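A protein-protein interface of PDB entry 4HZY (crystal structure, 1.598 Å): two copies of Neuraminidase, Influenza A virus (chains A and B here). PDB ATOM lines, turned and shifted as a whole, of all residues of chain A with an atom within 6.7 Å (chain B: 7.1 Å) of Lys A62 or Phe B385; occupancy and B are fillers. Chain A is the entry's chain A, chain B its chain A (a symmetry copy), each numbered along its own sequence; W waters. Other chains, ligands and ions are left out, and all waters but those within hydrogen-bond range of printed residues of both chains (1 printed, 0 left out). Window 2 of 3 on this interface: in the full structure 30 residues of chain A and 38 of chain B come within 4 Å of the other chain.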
ATOM      1  N   LYS A  31      31.285 -11.897  27.789  1.00  0.00           N
ATOM      2  CA  LYS A  31      30.808 -10.516  27.992  1.00  0.00           C
ATOM      3  C   LYS A  31      31.884  -9.530  28.453  1.00  0.00           C
ATOM      4  O   LYS A  31      31.570  -8.510  29.077  1.00  0.00           O
ATOM      5  CB  LYS A  31      29.601 -10.479  28.945  1.00  0.00           C
ATOM      6  CG  LYS A  31      28.448 -11.384  28.510  1.00  0.00           C
ATOM      7  CD  LYS A  31      27.231 -11.236  29.409  1.00  0.00           C
ATOM      8  CE  LYS A  31      26.150 -12.219  29.001  1.00  0.00           C
ATOM      9  NZ  LYS A  31      24.927 -12.095  29.849  1.00  0.00           N
ATOM     10  N   ALA A  57      28.633  -0.171  25.334  1.00  0.00           N
ATOM     11  CA  ALA A  57      28.038  -1.378  25.900  1.00  0.00           C
ATOM     12  C   ALA A  57      29.017  -2.536  25.751  1.00  0.00           C
ATOM     13  O   ALA A  57      29.861  -2.531  24.840  1.00  0.00           O
ATOM     14  CB  ALA A  57      26.734  -1.715  25.195  1.00  0.00           C
ATOM     15  N   LEU A  58      28.901  -3.518  26.644  1.00  0.00           N
ATOM     16  CA  LEU A  58      29.648  -4.755  26.507  1.00  0.00           C
ATOM     17  C   LEU A  58      28.871  -5.774  25.676  1.00  0.00           C
ATOM     18  O   LEU A  58      27.652  -5.890  25.771  1.00  0.00           O
ATOM     19  CB  LEU A  58      30.009  -5.340  27.874  1.00  0.00           C
ATOM     20  CG  LEU A  58      30.835  -4.422  28.769  1.00  0.00           C
ATOM     21  CD1 LEU A  58      31.138  -5.118  30.085  1.00  0.00           C
ATOM     22  CD2 LEU A  58      32.120  -3.987  28.079  1.00  0.00           C
ATOM     23  N   GLY A  60      27.029  -8.793  24.315  1.00  0.00           N
ATOM     24  CA  GLY A  60      26.227  -9.843  24.919  1.00  0.00           C
ATOM     25  C   GLY A  60      25.425  -9.384  26.127  1.00  0.00           C
ATOM     26  O   GLY A  60      24.646 -10.160  26.687  1.00  0.00           O
ATOM     27  N   THR A  61      25.609  -8.131  26.540  1.00  0.00           N
ATOM     28  CA  THR A  61      24.758  -7.571  27.584  1.00  0.00           C
ATOM     29  C   THR A  61      23.480  -7.029  26.964  1.00  0.00           C
ATOM     30  O   THR A  61      23.361  -6.935  25.741  1.00  0.00           O
ATOM     31  CB  THR A  61      25.448  -6.463  28.400  1.00  0.00           C
ATOM     32  OG1 THR A  61      25.721  -5.343  27.546  1.00  0.00           O
ATOM     33  CG2 THR A  61      26.739  -6.988  29.029  1.00  0.00           C
ATOM     34  N   LYS A  62      22.517  -6.681  27.806  1.00  0.00           N
ATOM     35  CA  LYS A  62      21.250  -6.151  27.308  1.00  0.00           C
ATOM     36  C   LYS A  62      21.417  -4.819  26.584  1.00  0.00           C
ATOM     37  O   LYS A  62      20.703  -4.536  25.615  1.00  0.00           O
ATOM     38  CB  LYS A  62      20.245  -6.021  28.453  1.00  0.00           C
ATOM     39  CG  LYS A  62      19.829  -7.360  29.055  1.00  0.00           C
ATOM     40  CD  LYS A  62      18.843  -7.134  30.201  1.00  0.00           C
ATOM     41  CE  LYS A  62      18.362  -8.448  30.799  1.00  0.00           C
ATOM     42  NZ  LYS A  62      19.491  -9.216  31.376  1.00  0.00           N
ATOM     43  N   HIS A  63      22.381  -4.012  27.023  1.00  0.00           N
ATOM     44  CA  HIS A  63      22.634  -2.748  26.341  1.00  0.00           C
ATOM     45  C   HIS A  63      23.235  -2.940  24.945  1.00  0.00           C
ATOM     46  O   HIS A  63      23.252  -2.003  24.158  1.00  0.00           O
ATOM     47  CB  HIS A  63      23.533  -1.823  27.179  1.00  0.00           C
ATOM     48  CG  HIS A  63      22.811  -1.126  28.293  1.00  0.00           C
ATOM     49  ND1 HIS A  63      22.818  -1.604  29.591  1.00  0.00           N
ATOM     50  CD2 HIS A  63      22.062  -0.006  28.307  1.00  0.00           C
ATOM     51  CE1 HIS A  63      22.099  -0.802  30.350  1.00  0.00           C
ATOM     52  NE2 HIS A  63      21.626   0.181  29.605  1.00  0.00           N
ATOM     53  N   SER A  64      23.721  -4.141  24.635  1.00  0.00           N
ATOM     54  CA  SER A  64      24.280  -4.381  23.301  1.00  0.00           C
ATOM     55  C   SER A  64      23.194  -4.673  22.264  1.00  0.00           C
ATOM     56  O   SER A  64      23.451  -4.645  21.061  1.00  0.00           O
ATOM     57  CB  SER A  64      25.342  -5.486  23.313  1.00  0.00           C
ATOM     58  OG  SER A  64      24.788  -6.781  23.480  1.00  0.00           O
ATOM     59  N   ASN A  65      21.978  -4.944  22.739  1.00  0.00           N
ATOM     60  CA  ASN A  65      20.846  -5.199  21.847  1.00  0.00           C
ATOM     61  C   ASN A  65      20.562  -3.944  21.019  1.00  0.00           C
ATOM     62  O   ASN A  65      20.382  -2.867  21.584  1.00  0.00           O
ATOM     63  CB  ASN A  65      19.628  -5.596  22.699  1.00  0.00           C
ATOM     64  CG  ASN A  65      18.441  -6.075  21.874  1.00  0.00           C
ATOM     65  OD1 ASN A  65      18.236  -5.651  20.729  1.00  0.00           O
ATOM     66  ND2 ASN A  65      17.644  -6.962  22.480  1.00  0.00           N
ATOM     67  N   GLY A  66      20.586  -4.067  19.689  1.00  0.00           N
ATOM     68  CA  GLY A  66      20.252  -2.954  18.802  1.00  0.00           C
ATOM     69  C   GLY A  66      21.404  -2.086  18.334  1.00  0.00           C
ATOM     70  O   GLY A  66      21.206  -1.017  17.743  1.00  0.00           O
ATOM     71  N   SER A 356      21.328 -10.190  18.875  1.00  0.00           N
ATOM     72  CA  SER A 356      20.660  -8.894  18.787  1.00  0.00           C
ATOM     73  C   SER A 356      21.635  -7.733  18.589  1.00  0.00           C
ATOM     74  O   SER A 356      21.218  -6.605  18.306  1.00  0.00           O
ATOM     75  CB  SER A 356      19.805  -8.636  20.031  1.00  0.00           C
ATOM     76  OG  SER A 356      20.622  -8.372  21.156  1.00  0.00           O
ATOM     77  N   LYS A 388      23.276 -13.683  23.199  1.00  0.00           N
ATOM     78  CA  LYS A 388      22.549 -12.984  22.151  1.00  0.00           C
ATOM     79  C   LYS A 388      22.285 -11.516  22.474  1.00  0.00           C
ATOM     80  O   LYS A 388      22.481 -11.046  23.604  1.00  0.00           O
ATOM     81  CB  LYS A 388      21.238 -13.714  21.852  1.00  0.00           C
ATOM     82  CG  LYS A 388      21.460 -15.126  21.316  1.00  0.00           C
ATOM     83  CD  LYS A 388      20.152 -15.784  20.904  1.00  0.00           C
ATOM     84  CE  LYS A 388      20.374 -17.248  20.559  1.00  0.00           C
ATOM     85  NZ  LYS A 388      21.282 -17.428  19.385  1.00  0.00           N
ATOM     86  OXT LYS A 388      21.867 -10.772  21.587  1.00  0.00           O
ATOM     87  N   GLU B  29      26.798  -2.976  33.432  1.00  0.00           N
ATOM     88  CA  GLU B  29      25.671  -3.898  33.504  1.00  0.00           C
ATOM     89  C   GLU B  29      26.096  -5.289  33.985  1.00  0.00           C
ATOM     90  O   GLU B  29      25.297  -6.002  34.590  1.00  0.00           O
ATOM     91  CB  GLU B  29      24.978  -3.992  32.136  1.00  0.00           C
ATOM     92  CG  GLU B  29      23.691  -4.805  32.133  1.00  0.00           C
ATOM     93  CD  GLU B  29      23.223  -5.128  30.726  1.00  0.00           C
ATOM     94  OE1 GLU B  29      23.361  -4.258  29.839  1.00  0.00           O
ATOM     95  OE2 GLU B  29      22.738  -6.258  30.516  1.00  0.00           O
ATOM     96  N   ASN B  30      27.345  -5.672  33.711  1.00  0.00           N
ATOM     97  CA  ASN B  30      27.826  -7.005  34.091  1.00  0.00           C
ATOM     98  C   ASN B  30      28.705  -6.979  35.346  1.00  0.00           C
ATOM     99  O   ASN B  30      29.500  -7.889  35.574  1.00  0.00           O
ATOM    100  CB  ASN B  30      28.540  -7.685  32.904  1.00  0.00           C
ATOM    101  CG  ASN B  30      28.637  -9.202  33.055  1.00  0.00           C
ATOM    102  OD1 ASN B  30      29.694  -9.793  32.817  1.00  0.00           O
ATOM    103  ND2 ASN B  30      27.543  -9.831  33.454  1.00  0.00           N
ATOM    104  N   SER B 381      21.707   4.807  30.238  1.00  0.00           N
ATOM    105  CA  SER B 381      21.414   3.460  30.724  1.00  0.00           C
ATOM    106  C   SER B 381      19.922   3.231  30.778  1.00  0.00           C
ATOM    107  O   SER B 381      19.166   4.136  31.121  1.00  0.00           O
ATOM    108  CB  SER B 381      21.995   3.252  32.125  1.00  0.00           C
ATOM    109  OG  SER B 381      23.368   3.564  32.119  1.00  0.00           O
ATOM    110  N   ASN B 382      19.514   2.013  30.434  1.00  0.00           N
ATOM    111  CA  ASN B 382      18.160   1.550  30.696  1.00  0.00           C
ATOM    112  C   ASN B 382      18.186   0.913  32.076  1.00  0.00           C
ATOM    113  O   ASN B 382      18.756  -0.157  32.265  1.00  0.00           O
ATOM    114  CB  ASN B 382      17.743   0.535  29.630  1.00  0.00           C
ATOM    115  CG  ASN B 382      16.303   0.111  29.775  1.00  0.00           C
ATOM    116  OD1 ASN B 382      15.796  -0.024  30.890  1.00  0.00           O
ATOM    117  ND2 ASN B 382      15.629  -0.097  28.650  1.00  0.00           N
ATOM    118  N   ILE B 383      17.626   1.595  33.063  1.00  0.00           N
ATOM    119  CA  ILE B 383      17.765   1.136  34.432  1.00  0.00           C
ATOM    120  C   ILE B 383      17.170  -0.258  34.633  1.00  0.00           C
ATOM    121  O   ILE B 383      17.608  -1.016  35.504  1.00  0.00           O
ATOM    122  CB  ILE B 383      17.181   2.156  35.442  1.00  0.00           C
ATOM    123  CG1 ILE B 383      17.799   1.940  36.818  1.00  0.00           C
ATOM    124  CG2 ILE B 383      15.663   2.090  35.483  1.00  0.00           C
ATOM    125  CD1 ILE B 383      19.230   2.416  36.902  1.00  0.00           C
ATOM    126  N   GLY B 384      16.193  -0.602  33.804  1.00  0.00           N
ATOM    127  CA  GLY B 384      15.573  -1.913  33.882  1.00  0.00           C
ATOM    128  C   GLY B 384      16.479  -3.046  33.429  1.00  0.00           C
ATOM    129  O   GLY B 384      16.184  -4.211  33.701  1.00  0.00           O
ATOM    130  N   PHE B 385      17.572  -2.721  32.733  1.00  0.00           N
ATOM    131  CA  PHE B 385      18.543  -3.741  32.326  1.00  0.00           C
ATOM    132  C   PHE B 385      19.563  -4.022  33.427  1.00  0.00           C
ATOM    133  O   PHE B 385      20.326  -4.986  33.340  1.00  0.00           O
ATOM    134  CB  PHE B 385      19.349  -3.305  31.090  1.00  0.00           C
ATOM    135  CG  PHE B 385      18.569  -3.243  29.812  1.00  0.00           C
ATOM    136  CD1 PHE B 385      17.302  -3.790  29.715  1.00  0.00           C
ATOM    137  CD2 PHE B 385      19.132  -2.650  28.686  1.00  0.00           C
ATOM    138  CE1 PHE B 385      16.598  -3.731  28.514  1.00  0.00           C
ATOM    139  CE2 PHE B 385      18.434  -2.581  27.486  1.00  0.00           C
ATOM    140  CZ  PHE B 385      17.168  -3.121  27.402  1.00  0.00           C
ATOM    141  N   MET B 386      19.606  -3.172  34.454  1.00  0.00           N
ATOM    142  CA  MET B 386      20.701  -3.223  35.424  1.00  0.00           C
ATOM    143  C   MET B 386      20.467  -4.191  36.573  1.00  0.00           C
ATOM    144  O   MET B 386      19.344  -4.342  37.042  1.00  0.00           O
ATOM    145  CB  MET B 386      20.965  -1.832  36.013  1.00  0.00           C
ATOM    146  CG  MET B 386      21.348  -0.767  34.995  1.00  0.00           C
ATOM    147  SD  MET B 386      22.865  -1.127  34.095  1.00  0.00           S
ATOM    148  CE  MET B 386      24.099  -0.989  35.398  1.00  0.00           C
ATOM    149  N   PRO B 387      21.541  -4.846  37.042  1.00  0.00           N
ATOM    150  CA  PRO B 387      21.443  -5.588  38.301  1.00  0.00           C
ATOM    151  C   PRO B 387      21.075  -4.602  39.403  1.00  0.00           C
ATOM    152  O   PRO B 387      21.639  -3.508  39.443  1.00  0.00           O
ATOM    153  CB  PRO B 387      22.866  -6.123  38.504  1.00  0.00           C
ATOM    154  CG  PRO B 387      23.740  -5.179  37.731  1.00  0.00           C
ATOM    155  CD  PRO B 387      22.917  -4.804  36.518  1.00  0.00           C
ATOM    156  N   LYS B 388      20.145  -4.976  40.273  1.00  0.00           N
ATOM    157  CA  LYS B 388      19.617  -4.046  41.258  1.00  0.00           C
ATOM    158  C   LYS B 388      20.481  -3.937  42.511  1.00  0.00           C
ATOM    159  O   LYS B 388      21.409  -4.725  42.740  1.00  0.00           O
ATOM    160  CB  LYS B 388      18.183  -4.437  41.625  1.00  0.00           C
ATOM    161  CG  LYS B 388      17.228  -4.351  40.437  1.00  0.00           C
ATOM    162  CD  LYS B 388      15.789  -4.616  40.852  1.00  0.00           C
ATOM    163  CE  LYS B 388      14.890  -4.718  39.631  1.00  0.00           C
ATOM    164  NZ  LYS B 388      14.837  -3.444  38.851  1.00  0.00           N
ATOM    165  OXT LYS B 388      20.255  -3.037  43.320  1.00  0.00           O
HETATM  166  O   HOH W   1      31.911  -8.435  31.865  1.00  0.00           O
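Printed residues of chain B within 4 Å of Lys A31: Asn B30. Leu A58 touches none of the printed residues of chain B. Printed residues of chain B within 4 Å of Thr A61: Glu B29. Lys A62 touches two residues of chain B. Ser A64 touches none of the printed residues of chain B. Of the printed residues of chain A, Asn B30 touches Lys A31. Phe B385 touches just these residues of chain A: Lys A62 and His A63. The nearest residue of chain A that does not touch Phe B385 is Asn A65 (5.8 Å).
OE2 of Glu B29 lies within hydrogen-bond range of N of Lys A62. OE1 of Glu B29 sits at hydrogen-bond distance from ND1 of His A63 (2.7 Å). N of Asn B382 is in hydrogen-bond range of NE2 of His A63 (2.9 Å). OE1 of Glu B29 sits close to OG1 of Thr A61, 3.5 Å away.
The side-chain amide oxygen (OD1) of Asn B382 sits at hydrogen-bond distance from the backbone NH (N) of Gly B384, 3.0 Å away. The side-chain hydroxyl (OG1) of Thr A61 is in hydrogen-bond range of the backbone carbonyl oxygen (O) of Leu A58 (2.7 Å). The backbone carbonyl oxygen (O) of Thr A61 sits at hydrogen-bond distance from the side-chain hydroxyl (OG) of Ser A64.
Position printed for both chains: 388.
Water W1 bridges the side-chain amide oxygen (OD1) of Asn B30 (2.8 Å) and the backbone carbonyl oxygen (O) of Lys A31 (2.8 Å).
Printed residues of chain B that touch a printed residue of chain A: Glu B29, Asn B30, Ser B381, Asn B382, Phe B385 and Met B386. Hydrophobic or aromatic side chains of chain B within 4 Å of the printed part of chain A: Phe B385 and Met B386. Of the 12 printed residues of chain A, 4 touch a printed residue of chain B. Hydrophobic or aromatic side chains of chain A within 4 Å of the printed part of chain B: His A63.
Lys A31 touches Asn B30 (CB to OD1, 3.9 Å). Phe B385 touches Lys A62. His A63 touches Ser B381 (NE2 to CA, 3.5 Å). His A63 touches Phe B385 (CE1 to CB, 3.8 Å). CE1 of His A63 touches SD of Met B386, at 3.8 Å.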
